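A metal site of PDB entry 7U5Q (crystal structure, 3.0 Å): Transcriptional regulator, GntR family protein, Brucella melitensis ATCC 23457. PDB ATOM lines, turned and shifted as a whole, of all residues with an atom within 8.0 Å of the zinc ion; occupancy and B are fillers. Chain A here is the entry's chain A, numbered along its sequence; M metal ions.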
ATOM      1  N   ARG A 129     -12.000 -12.586  26.422  1.00  0.00           N
ATOM      2  CA  ARG A 129     -10.928 -12.285  25.478  1.00  0.00           C
ATOM      3  C   ARG A 129      -9.600 -12.880  25.938  1.00  0.00           C
ATOM      4  O   ARG A 129      -8.872 -13.464  25.133  1.00  0.00           O
ATOM      5  CB  ARG A 129     -10.816 -10.783  25.267  1.00  0.00           C
ATOM      6  CG  ARG A 129     -10.183 -10.403  23.950  1.00  0.00           C
ATOM      7  CD  ARG A 129     -10.026  -8.906  23.789  1.00  0.00           C
ATOM      8  NE  ARG A 129      -9.199  -8.598  22.634  1.00  0.00           N
ATOM      9  CZ  ARG A 129      -8.818  -7.390  22.263  1.00  0.00           C
ATOM     10  NH1 ARG A 129      -9.154  -6.307  22.961  1.00  0.00           N
ATOM     11  NH2 ARG A 129      -8.074  -7.243  21.163  1.00  0.00           N
ATOM     12  N   GLU A 133      -8.190 -15.361  23.258  1.00  0.00           N
ATOM     13  CA  GLU A 133      -6.921 -14.913  22.685  1.00  0.00           C
ATOM     14  C   GLU A 133      -5.750 -15.578  23.389  1.00  0.00           C
ATOM     15  O   GLU A 133      -4.663 -15.694  22.797  1.00  0.00           O
ATOM     16  CB  GLU A 133      -6.799 -13.403  22.762  1.00  0.00           C
ATOM     17  CG  GLU A 133      -7.777 -12.682  21.853  1.00  0.00           C
ATOM     18  CD  GLU A 133      -7.098 -11.640  20.989  1.00  0.00           C
ATOM     19  OE1 GLU A 133      -5.908 -11.834  20.672  1.00  0.00           O
ATOM     20  OE2 GLU A 133      -7.754 -10.632  20.639  1.00  0.00           O
ATOM     21  N   GLN A 159       2.266  -0.467  12.797  1.00  0.00           N
ATOM     22  CA  GLN A 159       1.777   0.201  13.996  1.00  0.00           C
ATOM     23  C   GLN A 159       2.748   1.275  14.447  1.00  0.00           C
ATOM     24  O   GLN A 159       2.354   2.406  14.766  1.00  0.00           O
ATOM     25  CB  GLN A 159       1.554  -0.810  15.121  1.00  0.00           C
ATOM     26  CG  GLN A 159       0.176  -1.422  15.171  1.00  0.00           C
ATOM     27  CD  GLN A 159       0.077  -2.521  16.207  1.00  0.00           C
ATOM     28  OE1 GLN A 159      -0.607  -2.374  17.222  1.00  0.00           O
ATOM     29  NE2 GLN A 159       0.762  -3.643  15.967  1.00  0.00           N
ATOM     30  N   PHE A 171      -3.796   3.242  13.918  1.00  0.00           N
ATOM     31  CA  PHE A 171      -3.124   2.421  14.927  1.00  0.00           C
ATOM     32  C   PHE A 171      -4.077   1.383  15.513  1.00  0.00           C
ATOM     33  O   PHE A 171      -3.685   0.234  15.747  1.00  0.00           O
ATOM     34  CB  PHE A 171      -2.559   3.285  16.057  1.00  0.00           C
ATOM     35  CG  PHE A 171      -1.690   2.512  17.013  1.00  0.00           C
ATOM     36  CD1 PHE A 171      -2.245   1.823  18.088  1.00  0.00           C
ATOM     37  CD2 PHE A 171      -0.323   2.440  16.828  1.00  0.00           C
ATOM     38  CE1 PHE A 171      -1.460   1.092  18.949  1.00  0.00           C
ATOM     39  CE2 PHE A 171       0.471   1.707  17.692  1.00  0.00           C
ATOM     40  CZ  PHE A 171      -0.097   1.033  18.752  1.00  0.00           C
ATOM     41  N   HIS A 172      -5.323   1.780  15.785  1.00  0.00           N
ATOM     42  CA  HIS A 172      -6.266   0.828  16.340  1.00  0.00           C
ATOM     43  C   HIS A 172      -6.617  -0.247  15.321  1.00  0.00           C
ATOM     44  O   HIS A 172      -6.740  -1.423  15.673  1.00  0.00           O
ATOM     45  CB  HIS A 172      -7.526   1.536  16.837  1.00  0.00           C
ATOM     46  CG  HIS A 172      -8.273   0.772  17.878  1.00  0.00           C
ATOM     47  ND1 HIS A 172      -8.932  -0.416  17.600  1.00  0.00           N
ATOM     48  CD2 HIS A 172      -8.471   1.010  19.195  1.00  0.00           C
ATOM     49  CE1 HIS A 172      -9.500  -0.872  18.706  1.00  0.00           C
ATOM     50  NE2 HIS A 172      -9.232  -0.023  19.687  1.00  0.00           N
ATOM     51  N   THR A 174      -4.738  -1.368  12.836  1.00  0.00           N
ATOM     52  CA  THR A 174      -3.619  -2.294  12.703  1.00  0.00           C
ATOM     53  C   THR A 174      -3.478  -3.161  13.942  1.00  0.00           C
ATOM     54  O   THR A 174      -2.945  -4.277  13.868  1.00  0.00           O
ATOM     55  CB  THR A 174      -2.331  -1.531  12.413  1.00  0.00           C
ATOM     56  OG1 THR A 174      -2.557  -0.590  11.353  1.00  0.00           O
ATOM     57  CG2 THR A 174      -1.217  -2.478  12.003  1.00  0.00           C
ATOM     58  N   ASP A 175      -3.921  -2.648  15.099  1.00  0.00           N
ATOM     59  CA  ASP A 175      -4.016  -3.476  16.287  1.00  0.00           C
ATOM     60  C   ASP A 175      -4.915  -4.682  16.048  1.00  0.00           C
ATOM     61  O   ASP A 175      -4.540  -5.826  16.329  1.00  0.00           O
ATOM     62  CB  ASP A 175      -4.507  -2.628  17.461  1.00  0.00           C
ATOM     63  CG  ASP A 175      -4.132  -3.213  18.808  1.00  0.00           C
ATOM     64  OD1 ASP A 175      -3.707  -4.382  18.836  1.00  0.00           O
ATOM     65  OD2 ASP A 175      -4.236  -2.507  19.835  1.00  0.00           O
ATOM     66  N   ASP A 176      -6.121  -4.448  15.533  1.00  0.00           N
ATOM     67  CA  ASP A 176      -7.029  -5.546  15.215  1.00  0.00           C
ATOM     68  C   ASP A 176      -6.394  -6.526  14.239  1.00  0.00           C
ATOM     69  O   ASP A 176      -6.491  -7.747  14.412  1.00  0.00           O
ATOM     70  CB  ASP A 176      -8.343  -5.008  14.656  1.00  0.00           C
ATOM     71  CG  ASP A 176      -9.251  -4.421  15.724  1.00  0.00           C
ATOM     72  OD1 ASP A 176      -9.124  -4.800  16.902  1.00  0.00           O
ATOM     73  OD2 ASP A 176     -10.082  -3.548  15.373  1.00  0.00           O
ATOM     74  N   PHE A 178      -3.274  -7.169  13.813  1.00  0.00           N
ATOM     75  CA  PHE A 178      -2.233  -7.933  14.504  1.00  0.00           C
ATOM     76  C   PHE A 178      -2.833  -9.144  15.208  1.00  0.00           C
ATOM     77  O   PHE A 178      -2.304 -10.248  15.123  1.00  0.00           O
ATOM     78  CB  PHE A 178      -1.506  -7.030  15.499  1.00  0.00           C
ATOM     79  CG  PHE A 178      -0.448  -7.738  16.324  1.00  0.00           C
ATOM     80  CD1 PHE A 178       0.843  -7.869  15.849  1.00  0.00           C
ATOM     81  CD2 PHE A 178      -0.743  -8.227  17.585  1.00  0.00           C
ATOM     82  CE1 PHE A 178       1.822  -8.492  16.618  1.00  0.00           C
ATOM     83  CE2 PHE A 178       0.226  -8.858  18.349  1.00  0.00           C
ATOM     84  CZ  PHE A 178       1.507  -8.986  17.870  1.00  0.00           C
ATOM     85  N   HIS A 179      -3.946  -8.942  15.918  1.00  0.00           N
ATOM     86  CA  HIS A 179      -4.607 -10.040  16.620  1.00  0.00           C
ATOM     87  C   HIS A 179      -5.277 -10.997  15.643  1.00  0.00           C
ATOM     88  O   HIS A 179      -5.238 -12.213  15.841  1.00  0.00           O
ATOM     89  CB  HIS A 179      -5.619  -9.462  17.610  1.00  0.00           C
ATOM     90  CG  HIS A 179      -4.975  -8.795  18.784  1.00  0.00           C
ATOM     91  ND1 HIS A 179      -4.490  -9.486  19.872  1.00  0.00           N
ATOM     92  CD2 HIS A 179      -4.681  -7.492  18.998  1.00  0.00           C
ATOM     93  CE1 HIS A 179      -3.963  -8.628  20.733  1.00  0.00           C
ATOM     94  NE2 HIS A 179      -4.058  -7.418  20.228  1.00  0.00           N
ATOM     95  N   TRP A 192     -11.313 -15.008  15.919  1.00  0.00           N
ATOM     96  CA  TRP A 192     -11.252 -13.556  15.865  1.00  0.00           C
ATOM     97  C   TRP A 192     -12.607 -12.954  15.504  1.00  0.00           C
ATOM     98  O   TRP A 192     -13.068 -12.016  16.155  1.00  0.00           O
ATOM     99  CB  TRP A 192     -10.196 -13.107  14.855  1.00  0.00           C
ATOM    100  CG  TRP A 192     -10.160 -11.630  14.739  1.00  0.00           C
ATOM    101  CD1 TRP A 192     -10.496 -10.880  13.645  1.00  0.00           C
ATOM    102  CD2 TRP A 192      -9.829 -10.699  15.778  1.00  0.00           C
ATOM    103  NE1 TRP A 192     -10.358  -9.545  13.938  1.00  0.00           N
ATOM    104  CE2 TRP A 192      -9.955  -9.405  15.235  1.00  0.00           C
ATOM    105  CE3 TRP A 192      -9.430 -10.843  17.108  1.00  0.00           C
ATOM    106  CZ2 TRP A 192      -9.688  -8.266  15.976  1.00  0.00           C
ATOM    107  CZ3 TRP A 192      -9.162  -9.704  17.848  1.00  0.00           C
ATOM    108  CH2 TRP A 192      -9.295  -8.435  17.278  1.00  0.00           C
ATOM    109  N   ARG A 206     -10.984   1.926  24.586  1.00  0.00           N
ATOM    110  CA  ARG A 206      -9.615   2.071  24.109  1.00  0.00           C
ATOM    111  C   ARG A 206      -9.464   3.198  23.098  1.00  0.00           C
ATOM    112  O   ARG A 206      -8.362   3.731  22.945  1.00  0.00           O
ATOM    113  CB  ARG A 206      -9.079   0.751  23.567  1.00  0.00           C
ATOM    114  CG  ARG A 206      -8.706  -0.150  24.726  1.00  0.00           C
ATOM    115  CD  ARG A 206      -8.164  -1.501  24.346  1.00  0.00           C
ATOM    116  NE  ARG A 206      -6.978  -1.383  23.506  1.00  0.00           N
ATOM    117  CZ  ARG A 206      -6.324  -2.417  22.980  1.00  0.00           C
ATOM    118  NH1 ARG A 206      -6.719  -3.658  23.200  1.00  0.00           N
ATOM    119  NH2 ARG A 206      -5.240  -2.187  22.240  1.00  0.00           N
ATOM    120  N   MET A 210      -5.955   5.517  23.818  1.00  0.00           N
ATOM    121  CA  MET A 210      -4.817   5.543  22.904  1.00  0.00           C
ATOM    122  C   MET A 210      -4.173   6.930  22.783  1.00  0.00           C
ATOM    123  O   MET A 210      -2.939   7.013  22.886  1.00  0.00           O
ATOM    124  CB  MET A 210      -5.243   4.999  21.530  1.00  0.00           C
ATOM    125  CG  MET A 210      -5.433   3.507  21.470  1.00  0.00           C
ATOM    126  SD  MET A 210      -3.923   2.627  21.910  1.00  0.00           S
ATOM    127  CE  MET A 210      -4.369   1.909  23.497  1.00  0.00           C
ATOM    128  N   VAL A 219       1.602  -0.223  23.930  1.00  0.00           N
ATOM    129  CA  VAL A 219       1.000  -1.300  23.154  1.00  0.00           C
ATOM    130  C   VAL A 219       2.049  -1.978  22.288  1.00  0.00           C
ATOM    131  O   VAL A 219       2.098  -3.215  22.194  1.00  0.00           O
ATOM    132  CB  VAL A 219      -0.181  -0.763  22.313  1.00  0.00           C
ATOM    133  CG1 VAL A 219      -0.684  -1.837  21.372  1.00  0.00           C
ATOM    134  CG2 VAL A 219      -1.294  -0.255  23.210  1.00  0.00           C
ATOM    135  N   LEU A 220       2.898  -1.186  21.621  1.00  0.00           N
ATOM    136  CA  LEU A 220       3.949  -1.757  20.789  1.00  0.00           C
ATOM    137  C   LEU A 220       4.893  -2.640  21.602  1.00  0.00           C
ATOM    138  O   LEU A 220       5.293  -3.719  21.160  1.00  0.00           O
ATOM    139  CB  LEU A 220       4.727  -0.655  20.072  1.00  0.00           C
ATOM    140  CG  LEU A 220       4.035  -0.002  18.872  1.00  0.00           C
ATOM    141  CD1 LEU A 220       4.796   1.235  18.446  1.00  0.00           C
ATOM    142  CD2 LEU A 220       3.932  -0.950  17.720  1.00  0.00           C
ATOM    143  N   GLU A 222       4.092  -4.270  24.290  1.00  0.00           N
ATOM    144  CA  GLU A 222       3.343  -5.481  24.615  1.00  0.00           C
ATOM    145  C   GLU A 222       3.244  -6.400  23.414  1.00  0.00           C
ATOM    146  O   GLU A 222       3.326  -7.624  23.553  1.00  0.00           O
ATOM    147  CB  GLU A 222       1.965  -5.101  25.157  1.00  0.00           C
ATOM    148  CG  GLU A 222       2.039  -4.322  26.474  1.00  0.00           C
ATOM    149  CD  GLU A 222       0.710  -3.748  26.927  1.00  0.00           C
ATOM    150  OE1 GLU A 222      -0.261  -3.771  26.134  1.00  0.00           O
ATOM    151  OE2 GLU A 222       0.647  -3.234  28.070  1.00  0.00           O
ATOM    152  N   HIS A 223       3.049  -5.831  22.217  1.00  0.00           N
ATOM    153  CA  HIS A 223       3.016  -6.635  21.002  1.00  0.00           C
ATOM    154  C   HIS A 223       4.359  -7.316  20.728  1.00  0.00           C
ATOM    155  O   HIS A 223       4.394  -8.465  20.277  1.00  0.00           O
ATOM    156  CB  HIS A 223       2.589  -5.771  19.816  1.00  0.00           C
ATOM    157  CG  HIS A 223       1.110  -5.559  19.730  1.00  0.00           C
ATOM    158  ND1 HIS A 223       0.518  -4.878  18.684  1.00  0.00           N
ATOM    159  CD2 HIS A 223       0.113  -5.922  20.557  1.00  0.00           C
ATOM    160  CE1 HIS A 223      -0.782  -4.848  18.870  1.00  0.00           C
ATOM    161  NE2 HIS A 223      -1.059  -5.471  20.004  1.00  0.00           N
ATOM    162  N   ILE A 226       4.512 -10.424  22.727  1.00  0.00           N
ATOM    163  CA  ILE A 226       3.698 -11.506  22.178  1.00  0.00           C
ATOM    164  C   ILE A 226       4.366 -12.116  20.952  1.00  0.00           C
ATOM    165  O   ILE A 226       4.393 -13.337  20.784  1.00  0.00           O
ATOM    166  CB  ILE A 226       2.279 -11.005  21.865  1.00  0.00           C
ATOM    167  CG1 ILE A 226       1.567 -10.605  23.158  1.00  0.00           C
ATOM    168  CG2 ILE A 226       1.491 -12.080  21.142  1.00  0.00           C
ATOM    169  CD1 ILE A 226       0.284  -9.821  22.923  1.00  0.00           C
ATOM    170  N   MET A 242      -0.028 -12.514  26.071  1.00  0.00           N
ATOM    171  CA  MET A 242      -1.301 -12.094  25.505  1.00  0.00           C
ATOM    172  C   MET A 242      -2.301 -11.745  26.606  1.00  0.00           C
ATOM    173  O   MET A 242      -3.016 -10.743  26.514  1.00  0.00           O
ATOM    174  CB  MET A 242      -1.862 -13.183  24.592  1.00  0.00           C
ATOM    175  CG  MET A 242      -3.246 -12.919  24.072  1.00  0.00           C
ATOM    176  SD  MET A 242      -3.280 -11.532  22.935  1.00  0.00           S
ATOM    177  CE  MET A 242      -2.368 -12.193  21.533  1.00  0.00           C
ATOM    178  N   HIS A 245      -1.141  -8.236  28.225  1.00  0.00           N
ATOM    179  CA  HIS A 245      -1.518  -7.206  27.264  1.00  0.00           C
ATOM    180  C   HIS A 245      -3.008  -6.852  27.320  1.00  0.00           C
ATOM    181  O   HIS A 245      -3.369  -5.671  27.277  1.00  0.00           O
ATOM    182  CB  HIS A 245      -1.146  -7.683  25.863  1.00  0.00           C
ATOM    183  CG  HIS A 245      -1.740  -6.869  24.765  1.00  0.00           C
ATOM    184  ND1 HIS A 245      -1.513  -5.521  24.617  1.00  0.00           N
ATOM    185  CD2 HIS A 245      -2.602  -7.225  23.774  1.00  0.00           C
ATOM    186  CE1 HIS A 245      -2.183  -5.084  23.566  1.00  0.00           C
ATOM    187  NE2 HIS A 245      -2.856  -6.091  23.040  1.00  0.00           N
ATOM    188  N   LEU A 246      -3.864  -7.861  27.426  1.00  0.00           N
ATOM    189  CA  LEU A 246      -5.308  -7.634  27.399  1.00  0.00           C
ATOM    190  C   LEU A 246      -5.860  -7.089  28.711  1.00  0.00           C
ATOM    191  O   LEU A 246      -6.950  -6.526  28.718  1.00  0.00           O
ATOM    192  CB  LEU A 246      -6.033  -8.928  27.027  1.00  0.00           C
ATOM    193  CG  LEU A 246      -5.804  -9.440  25.605  1.00  0.00           C
ATOM    194  CD1 LEU A 246      -6.454 -10.801  25.421  1.00  0.00           C
ATOM    195  CD2 LEU A 246      -6.343  -8.453  24.583  1.00  0.00           C
HETATM  196 ZN    ZN M   1      -3.188  -5.380  20.907  1.00  0.00          ZN
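The zinc ion is bound by NE2 of His 245 (2.3 Å).
NE2 of His 223 binds the zinc ion (2.3 Å).
NE2 of His 179 is bound to the zinc ion (2.3 Å).
The zinc ion is bound by OD1 of Asp 175 (2.4 Å).
The side-chain carboxylate of Glu 222 is in hydrogen-bond range of a ring nitrogen (ND1) of His 245 (2.6 Å).
The side-chain amide nitrogen of Gln 159 lies within hydrogen-bond range of a ring nitrogen (ND1) of His 223 (3.0 Å).
A ring nitrogen (ND1) of His 179 sits at hydrogen-bond distance from the side-chain carboxylate (OE1) of Glu 133, at 2.9 Å.
The guanidinium group (NH2) of Arg 206 lies within salt-bridge range of the side-chain carboxylate (OD2) of Asp 175, 2.6 Å away.
The nearest printed residue that does not touch the zinc ion is Arg 206 (4.02 Å).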
